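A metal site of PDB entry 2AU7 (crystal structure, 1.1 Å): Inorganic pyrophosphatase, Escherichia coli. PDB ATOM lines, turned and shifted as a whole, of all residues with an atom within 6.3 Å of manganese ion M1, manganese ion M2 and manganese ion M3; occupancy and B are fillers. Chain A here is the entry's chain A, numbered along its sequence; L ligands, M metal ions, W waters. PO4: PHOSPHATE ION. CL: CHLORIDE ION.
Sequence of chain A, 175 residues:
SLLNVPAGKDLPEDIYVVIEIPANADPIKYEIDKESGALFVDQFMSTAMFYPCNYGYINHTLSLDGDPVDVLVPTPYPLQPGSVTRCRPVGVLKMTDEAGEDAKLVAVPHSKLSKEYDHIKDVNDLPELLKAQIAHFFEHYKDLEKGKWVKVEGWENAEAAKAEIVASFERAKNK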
ATOM      1  N   GLU A  20       1.703   7.402 -36.022  1.00  0.00           N
ATOM      2  CA  GLU A  20       0.403   7.451 -35.393  1.00  0.00           C
ATOM      3  C   GLU A  20      -0.500   8.535 -35.977  1.00  0.00           C
ATOM      4  O   GLU A  20      -1.720   8.326 -36.036  1.00  0.00           O
ATOM      5  CB  GLU A  20       0.545   7.674 -33.889  1.00  0.00           C
ATOM      6  CG  GLU A  20       1.156   6.433 -33.204  1.00  0.00           C
ATOM      7  CD  GLU A  20       1.624   6.645 -31.810  1.00  0.00           C
ATOM      8  OE1 GLU A  20       2.205   7.732 -31.600  1.00  0.00           O
ATOM      9  OE2 GLU A  20       1.462   5.715 -30.971  1.00  0.00           O
ATOM     10  N   LYS A  29      -5.496  12.791 -31.698  1.00  0.00           N
ATOM     11  CA  LYS A  29      -4.248  12.163 -31.260  1.00  0.00           C
ATOM     12  C   LYS A  29      -4.557  10.673 -31.170  1.00  0.00           C
ATOM     13  O   LYS A  29      -5.418  10.313 -30.405  1.00  0.00           O
ATOM     14  CB  LYS A  29      -3.776  12.713 -29.961  1.00  0.00           C
ATOM     15  CG  LYS A  29      -2.412  12.238 -29.478  1.00  0.00           C
ATOM     16  CD  LYS A  29      -1.957  12.674 -28.164  1.00  0.00           C
ATOM     17  CE  LYS A  29      -0.517  12.374 -27.888  1.00  0.00           C
ATOM     18  NZ  LYS A  29      -0.087  10.965 -27.919  1.00  0.00           N
ATOM     19  N   GLU A  31      -2.825   6.652 -30.607  1.00  0.00           N
ATOM     20  CA  GLU A  31      -1.682   5.936 -30.048  1.00  0.00           C
ATOM     21  C   GLU A  31      -1.811   4.465 -30.330  1.00  0.00           C
ATOM     22  O   GLU A  31      -2.902   3.906 -30.195  1.00  0.00           O
ATOM     23  CB  GLU A  31      -1.530   6.155 -28.535  1.00  0.00           C
ATOM     24  CG  GLU A  31      -1.219   7.644 -28.173  1.00  0.00           C
ATOM     25  CD  GLU A  31      -0.821   7.750 -26.692  1.00  0.00           C
ATOM     26  OE1 GLU A  31      -1.595   7.267 -25.810  1.00  0.00           O
ATOM     27  OE2 GLU A  31       0.224   8.265 -26.178  1.00  0.00           O
ATOM     28  N   TYR A  55       3.769  12.216 -37.008  1.00  0.00           N
ATOM     29  CA  TYR A  55       4.144  11.990 -35.635  1.00  0.00           C
ATOM     30  C   TYR A  55       3.995  10.540 -35.249  1.00  0.00           C
ATOM     31  O   TYR A  55       2.962   9.924 -35.556  1.00  0.00           O
ATOM     32  CB  TYR A  55       3.279  12.868 -34.732  1.00  0.00           C
ATOM     33  CG  TYR A  55       3.622  12.836 -33.236  1.00  0.00           C
ATOM     34  CD1 TYR A  55       4.692  13.522 -32.745  1.00  0.00           C
ATOM     35  CD2 TYR A  55       2.853  12.082 -32.362  1.00  0.00           C
ATOM     36  CE1 TYR A  55       5.034  13.510 -31.413  1.00  0.00           C
ATOM     37  CE2 TYR A  55       3.131  12.047 -31.011  1.00  0.00           C
ATOM     38  CZ  TYR A  55       4.248  12.778 -30.532  1.00  0.00           C
ATOM     39  OH  TYR A  55       4.547  12.803 -29.192  1.00  0.00           O
ATOM     40  N   GLY A  56       4.972  10.003 -34.557  1.00  0.00           N
ATOM     41  CA  GLY A  56       4.882   8.642 -34.079  1.00  0.00           C
ATOM     42  C   GLY A  56       5.992   8.328 -33.106  1.00  0.00           C
ATOM     43  O   GLY A  56       6.328   9.133 -32.248  1.00  0.00           O
ATOM     44  N   TYR A  57       6.599   7.122 -33.214  1.00  0.00           N
ATOM     45  CA  TYR A  57       7.535   6.657 -32.242  1.00  0.00           C
ATOM     46  C   TYR A  57       8.480   5.628 -32.828  1.00  0.00           C
ATOM     47  O   TYR A  57       8.257   5.083 -33.909  1.00  0.00           O
ATOM     48  CB  TYR A  57       6.782   6.058 -31.010  1.00  0.00           C
ATOM     49  CG  TYR A  57       5.978   4.812 -31.365  1.00  0.00           C
ATOM     50  CD1 TYR A  57       4.665   4.881 -31.850  1.00  0.00           C
ATOM     51  CD2 TYR A  57       6.515   3.556 -31.254  1.00  0.00           C
ATOM     52  CE1 TYR A  57       3.958   3.781 -32.188  1.00  0.00           C
ATOM     53  CE2 TYR A  57       5.810   2.410 -31.592  1.00  0.00           C
ATOM     54  CZ  TYR A  57       4.539   2.532 -32.068  1.00  0.00           C
ATOM     55  OH  TYR A  57       3.783   1.411 -32.415  1.00  0.00           O
ATOM     56  N   SER A  63      10.588   6.404 -23.242  1.00  0.00           N
ATOM     57  CA  SER A  63      10.889   7.678 -22.610  1.00  0.00           C
ATOM     58  C   SER A  63      10.415   7.596 -21.157  1.00  0.00           C
ATOM     59  O   SER A  63       9.693   6.687 -20.774  1.00  0.00           O
ATOM     60  CB  SER A  63      10.229   8.868 -23.296  1.00  0.00           C
ATOM     61  OG  SER A  63      10.860   9.091 -24.549  1.00  0.00           O
ATOM     62  N   ASP A  65       8.243   9.350 -19.878  1.00  0.00           N
ATOM     63  CA  ASP A  65       6.801   9.460 -19.817  1.00  0.00           C
ATOM     64  C   ASP A  65       6.067   8.144 -19.899  1.00  0.00           C
ATOM     65  O   ASP A  65       4.848   8.132 -19.848  1.00  0.00           O
ATOM     66  CB  ASP A  65       6.256  10.459 -20.877  1.00  0.00           C
ATOM     67  CG  ASP A  65       6.272   9.866 -22.290  1.00  0.00           C
ATOM     68  OD1 ASP A  65       5.529  10.462 -23.148  1.00  0.00           O
ATOM     69  OD2 ASP A  65       6.958   8.856 -22.566  1.00  0.00           O
ATOM     70  N   ASP A  67       6.073   5.917 -22.460  1.00  0.00           N
ATOM     71  CA  ASP A  67       5.701   5.536 -23.811  1.00  0.00           C
ATOM     72  C   ASP A  67       7.011   5.520 -24.652  1.00  0.00           C
ATOM     73  O   ASP A  67       7.962   6.208 -24.313  1.00  0.00           O
ATOM     74  CB  ASP A  67       4.886   6.718 -24.439  1.00  0.00           C
ATOM     75  CG  ASP A  67       3.516   7.159 -23.846  1.00  0.00           C
ATOM     76  OD1 ASP A  67       3.015   6.412 -22.990  1.00  0.00           O
ATOM     77  OD2 ASP A  67       2.896   8.238 -24.273  1.00  0.00           O
ATOM     78  N   PRO A  68       6.974   4.839 -25.796  1.00  0.00           N
ATOM     79  CA  PRO A  68       8.114   4.876 -26.725  1.00  0.00           C
ATOM     80  C   PRO A  68       8.494   6.291 -27.094  1.00  0.00           C
ATOM     81  O   PRO A  68       7.660   7.191 -27.125  1.00  0.00           O
ATOM     82  CB  PRO A  68       7.612   4.063 -27.904  1.00  0.00           C
ATOM     83  CG  PRO A  68       6.702   3.052 -27.282  1.00  0.00           C
ATOM     84  CD  PRO A  68       5.942   3.861 -26.262  1.00  0.00           C
ATOM     85  N   VAL A  69       9.778   6.490 -27.389  1.00  0.00           N
ATOM     86  CA  VAL A  69      10.266   7.860 -27.711  1.00  0.00           C
ATOM     87  C   VAL A  69       9.577   8.347 -28.973  1.00  0.00           C
ATOM     88  O   VAL A  69       9.368   7.628 -29.945  1.00  0.00           O
ATOM     89  CB  VAL A  69      11.804   7.884 -27.843  1.00  0.00           C
ATOM     90  CG1 VAL A  69      12.346   7.186 -29.058  1.00  0.00           C
ATOM     91  CG2 VAL A  69      12.343   9.334 -27.745  1.00  0.00           C
ATOM     92  N   ASP A  70       9.237   9.642 -28.903  1.00  0.00           N
ATOM     93  CA  ASP A  70       8.457  10.287 -29.937  1.00  0.00           C
ATOM     94  C   ASP A  70       9.304  10.857 -31.057  1.00  0.00           C
ATOM     95  O   ASP A  70      10.422  11.357 -30.824  1.00  0.00           O
ATOM     96  CB  ASP A  70       7.646  11.409 -29.276  1.00  0.00           C
ATOM     97  CG  ASP A  70       6.717  10.884 -28.222  1.00  0.00           C
ATOM     98  OD1 ASP A  70       6.047   9.874 -28.498  1.00  0.00           O
ATOM     99  OD2 ASP A  70       6.662  11.495 -27.137  1.00  0.00           O
ATOM    100  N   MET A  95      11.979  18.521 -23.995  1.00  0.00           N
ATOM    101  CA  MET A  95      10.810  19.003 -23.312  1.00  0.00           C
ATOM    102  C   MET A  95      10.298  17.941 -22.332  1.00  0.00           C
ATOM    103  O   MET A  95      10.642  16.751 -22.451  1.00  0.00           O
ATOM    104  CB  MET A  95       9.685  19.450 -24.290  1.00  0.00           C
ATOM    105  CG  MET A  95       9.272  18.331 -25.279  1.00  0.00           C
ATOM    106  SD  MET A  95       7.647  18.597 -26.005  1.00  0.00           S
ATOM    107  CE  MET A  95       6.677  17.844 -24.664  1.00  0.00           C
ATOM    108  N   ASP A  97       6.444  16.798 -20.282  1.00  0.00           N
ATOM    109  CA  ASP A  97       5.019  17.106 -20.073  1.00  0.00           C
ATOM    110  C   ASP A  97       4.610  16.470 -18.784  1.00  0.00           C
ATOM    111  O   ASP A  97       5.406  15.998 -17.966  1.00  0.00           O
ATOM    112  CB  ASP A  97       4.146  16.711 -21.254  1.00  0.00           C
ATOM    113  CG  ASP A  97       3.820  15.268 -21.494  1.00  0.00           C
ATOM    114  OD1 ASP A  97       4.282  14.360 -20.751  1.00  0.00           O
ATOM    115  OD2 ASP A  97       3.103  15.032 -22.532  1.00  0.00           O
ATOM    116  N   GLU A  98       3.309  16.486 -18.491  1.00  0.00           N
ATOM    117  CA  GLU A  98       2.786  16.060 -17.178  1.00  0.00           C
ATOM    118  C   GLU A  98       3.111  14.631 -16.908  1.00  0.00           C
ATOM    119  O   GLU A  98       3.084  14.241 -15.695  1.00  0.00           O
ATOM    120  CB  GLU A  98       1.292  16.296 -17.021  1.00  0.00           C
ATOM    121  CG  GLU A  98       0.387  15.407 -17.827  1.00  0.00           C
ATOM    122  CD  GLU A  98       0.403  15.623 -19.323  1.00  0.00           C
ATOM    123  OE1 GLU A  98       0.739  16.655 -19.845  1.00  0.00           O
ATOM    124  OE2 GLU A  98       0.046  14.593 -19.970  1.00  0.00           O
ATOM    125  N   ALA A  99       3.376  13.797 -17.921  1.00  0.00           N
ATOM    126  CA  ALA A  99       3.697  12.381 -17.738  1.00  0.00           C
ATOM    127  C   ALA A  99       5.180  12.114 -17.539  1.00  0.00           C
ATOM    128  O   ALA A  99       5.530  10.978 -17.124  1.00  0.00           O
ATOM    129  CB  ALA A  99       3.144  11.545 -18.861  1.00  0.00           C
ATOM    130  N   GLY A 100       6.053  13.079 -17.771  1.00  0.00           N
ATOM    131  CA  GLY A 100       7.486  12.934 -17.578  1.00  0.00           C
ATOM    132  C   GLY A 100       8.294  13.548 -18.702  1.00  0.00           C
ATOM    133  O   GLY A 100       7.731  14.198 -19.636  1.00  0.00           O
ATOM    134  N   GLU A 101       9.592  13.364 -18.638  1.00  0.00           N
ATOM    135  CA  GLU A 101      10.454  13.823 -19.732  1.00  0.00           C
ATOM    136  C   GLU A 101      10.017  13.149 -21.023  1.00  0.00           C
ATOM    137  O   GLU A 101       9.644  11.991 -21.043  1.00  0.00           O
ATOM    138  CB  GLU A 101      11.900  13.475 -19.397  1.00  0.00           C
ATOM    139  CG  GLU A 101      12.661  14.466 -18.577  1.00  0.00           C
ATOM    140  CD  GLU A 101      14.118  14.183 -18.303  1.00  0.00           C
ATOM    141  OE1 GLU A 101      14.468  14.593 -17.176  1.00  0.00           O
ATOM    142  OE2 GLU A 101      14.793  13.591 -19.144  1.00  0.00           O
ATOM    143  N   ASP A 102      10.030  13.996 -22.111  1.00  0.00           N
ATOM    144  CA  ASP A 102       9.198  13.638 -23.267  1.00  0.00           C
ATOM    145  C   ASP A 102       9.760  14.288 -24.511  1.00  0.00           C
ATOM    146  O   ASP A 102       9.061  15.015 -25.233  1.00  0.00           O
ATOM    147  CB  ASP A 102       7.764  14.082 -22.993  1.00  0.00           C
ATOM    148  CG  ASP A 102       6.697  13.530 -23.952  1.00  0.00           C
ATOM    149  OD1 ASP A 102       7.005  12.519 -24.608  1.00  0.00           O
ATOM    150  OD2 ASP A 102       5.603  14.152 -23.996  1.00  0.00           O
ATOM    151  N   ALA A 103      11.034  14.012 -24.814  1.00  0.00           N
ATOM    152  CA  ALA A 103      11.693  14.580 -25.958  1.00  0.00           C
ATOM    153  C   ALA A 103      10.990  14.266 -27.270  1.00  0.00           C
ATOM    154  O   ALA A 103      10.448  13.157 -27.455  1.00  0.00           O
ATOM    155  CB  ALA A 103      13.121  14.035 -26.040  1.00  0.00           C
ATOM    156  N   LYS A 104      11.085  15.185 -28.201  1.00  0.00           N
ATOM    157  CA  LYS A 104      10.551  15.009 -29.553  1.00  0.00           C
ATOM    158  C   LYS A 104      11.716  14.973 -30.549  1.00  0.00           C
ATOM    159  O   LYS A 104      12.301  16.017 -30.880  1.00  0.00           O
ATOM    160  CB  LYS A 104       9.564  16.151 -29.903  1.00  0.00           C
ATOM    161  CG  LYS A 104       8.503  16.367 -28.893  1.00  0.00           C
ATOM    162  CD  LYS A 104       7.636  15.143 -28.578  1.00  0.00           C
ATOM    163  CE  LYS A 104       6.623  15.439 -27.534  1.00  0.00           C
ATOM    164  NZ  LYS A 104       5.931  14.261 -27.033  1.00  0.00           N
ATOM    165  N   TYR A 141      -0.711  22.952 -27.426  1.00  0.00           N
ATOM    166  CA  TYR A 141      -1.822  22.128 -27.863  1.00  0.00           C
ATOM    167  C   TYR A 141      -2.658  21.627 -26.685  1.00  0.00           C
ATOM    168  O   TYR A 141      -3.865  21.321 -26.895  1.00  0.00           O
ATOM    169  CB  TYR A 141      -1.394  20.989 -28.798  1.00  0.00           C
ATOM    170  CG  TYR A 141      -0.931  19.695 -28.169  1.00  0.00           C
ATOM    171  CD1 TYR A 141       0.338  19.528 -27.644  1.00  0.00           C
ATOM    172  CD2 TYR A 141      -1.744  18.574 -28.140  1.00  0.00           C
ATOM    173  CE1 TYR A 141       0.759  18.312 -27.110  1.00  0.00           C
ATOM    174  CE2 TYR A 141      -1.348  17.390 -27.621  1.00  0.00           C
ATOM    175  CZ  TYR A 141      -0.096  17.258 -27.106  1.00  0.00           C
ATOM    176  OH  TYR A 141       0.283  16.019 -26.547  1.00  0.00           O
ATOM    177  N   LYS A 142      -2.073  21.529 -25.487  1.00  0.00           N
ATOM    178  CA  LYS A 142      -2.765  21.097 -24.285  1.00  0.00           C
ATOM    179  C   LYS A 142      -3.323  22.276 -23.442  1.00  0.00           C
ATOM    180  O   LYS A 142      -3.737  22.065 -22.278  1.00  0.00           O
ATOM    181  CB  LYS A 142      -1.804  20.422 -23.307  1.00  0.00           C
ATOM    182  CG  LYS A 142      -0.990  19.281 -23.894  1.00  0.00           C
ATOM    183  CD  LYS A 142       0.137  18.859 -23.026  1.00  0.00           C
ATOM    184  CE  LYS A 142       0.825  17.624 -23.535  1.00  0.00           C
ATOM    185  NZ  LYS A 142       0.690  16.438 -22.689  1.00  0.00           N
ATOM    186  N   VAL A 150       3.086  21.358 -20.834  1.00  0.00           N
ATOM    187  CA  VAL A 150       4.365  21.166 -21.432  1.00  0.00           C
ATOM    188  C   VAL A 150       5.355  22.239 -20.958  1.00  0.00           C
ATOM    189  O   VAL A 150       4.991  23.391 -20.834  1.00  0.00           O
ATOM    190  CB  VAL A 150       4.277  21.203 -23.009  1.00  0.00           C
ATOM    191  CG1 VAL A 150       5.628  21.309 -23.662  1.00  0.00           C
ATOM    192  CG2 VAL A 150       3.551  19.935 -23.480  1.00  0.00           C
HETATM  193  P   PO4 L   1       3.158  11.079 -26.275  1.00  0.00           P
HETATM  194  O1  PO4 L   1       1.760  10.969 -25.713  1.00  0.00           O
HETATM  195  O2  PO4 L   1       3.135  11.145 -27.792  1.00  0.00           O
HETATM  196  O3  PO4 L   1       3.965  12.209 -25.623  1.00  0.00           O
HETATM  197  O4  PO4 L   1       3.996   9.780 -25.956  1.00  0.00           O
HETATM  198 CL    CL L   2       3.326  15.739 -25.818  1.00  0.00          CL
HETATM  199 MN    MN M   1       5.812  10.900 -25.245  1.00  0.00          MN
HETATM  200 MN    MN M   2       4.129   9.104 -28.125  1.00  0.00          MN
HETATM  201 MN    MN M   3       3.525  13.777 -24.210  1.00  0.00          MN
HETATM  202 MN    MN M   4       0.637   9.600 -24.476  1.00  0.00          MN
HETATM  203  O   HOH W   1       4.966   7.137 -27.719  1.00  0.00           O
HETATM  204  O   HOH W   2       1.375  13.331 -24.427  1.00  0.00           O
HETATM  205  O   HOH W   3       4.102   8.870 -30.245  1.00  0.00           O
HETATM  206  O   HOH W   4       7.214   9.217 -25.249  1.00  0.00           O
HETATM  207  O   HOH W   5       3.684  12.261 -22.508  1.00  0.00           O
HETATM  208  O   HOH W   6       2.165   8.185 -28.174  1.00  0.00           O
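OD2 of Asp 102 sits close to NZ of Lys 104, 3.1 Å away.
The side-chain carboxylate (OD2) of Asp 65 is in hydrogen-bond range of the backbone NH (N) of Asp 67 (3.1 Å).
NZ of Lys 104 lies within hydrogen-bond range of OH of Tyr 55.
The side-chain carboxylate (OD2) of Asp 70 sits close to the side-chain amino group (NZ) of Lys 104 (2.9 Å).
OD1 of Asp 97 lies within hydrogen-bond range of N of Ala 99 (3.0 Å).
The side-chain hydroxyl (OH) of Tyr 55 sits close to the side-chain carboxylate (OD2) of Asp 70, at 3.2 Å.
O of Met 95 sits at hydrogen-bond distance from N of Asp 102 (2.8 Å).
The backbone carbonyl oxygen (O) of Tyr 55 is in hydrogen-bond range of the backbone NH (N) of Glu 20, 2.9 Å away.
Tyr 55 touches manganese ion M2.
Of the 24 residues printed, 2 come within 4 Å of manganese ion M2.
The nearest printed residue that does not touch manganese ion M2 is Asp 67 (4.1 Å).
Manganese ion M3 is bound by the side-chain carboxylate of Asp 102 (2.1 Å), the side-chain carboxylate of Asp 97 (2.1 Å), an oxygen (O3) of PO4 L1 (2.2 Å), water W2 (2.2 Å), water W5 (2.3 Å) and a chlorine (CL) of CL L2 (2.5 Å).
Manganese ion M3 has six donor atoms within binding distance.
OD1 of Asp 102 is bound to manganese ion M1, 2.1 Å away.
The side-chain carboxylate (OD2) of Asp 70 binds manganese ion M1.
Manganese ion M1 is bound by OD1 of Asp 65, at 2.2 Å.
Manganese ion M1 is bound by water W4 (2.2 Å).
O4 of PO4 L1 binds manganese ion M1 (2.2 Å).
O3 of PO4 L1 is bound to manganese ion M1.
Manganese ion M1 has six donor atoms within binding distance.
Merely in contact with manganese ion M1: Lys 104 (3.8 Å).
Along chain A the residues within 4 Å of manganese ion M1 span positions 65 to 104.
Lys 104 touches manganese ion M3.
Within 4 Å of manganese ion M3: Asp 97, Asp 102 and Lys 104.
Water W3 lies within hydrogen-bond range of the side-chain carboxylate (OE1) of Glu 20 and the backbone carbonyl oxygen (O) of Gly 56.
Manganese ion M2 is bound by the side-chain carboxylate of Asp 70 (2.1 Å), water W3 (2.1 Å), water W6 (2.2 Å), water W1 (2.2 Å), an oxygen (O4) of PO4 L1 (2.3 Å) and an oxygen (O2) of PO4 L1 (2.3 Å).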
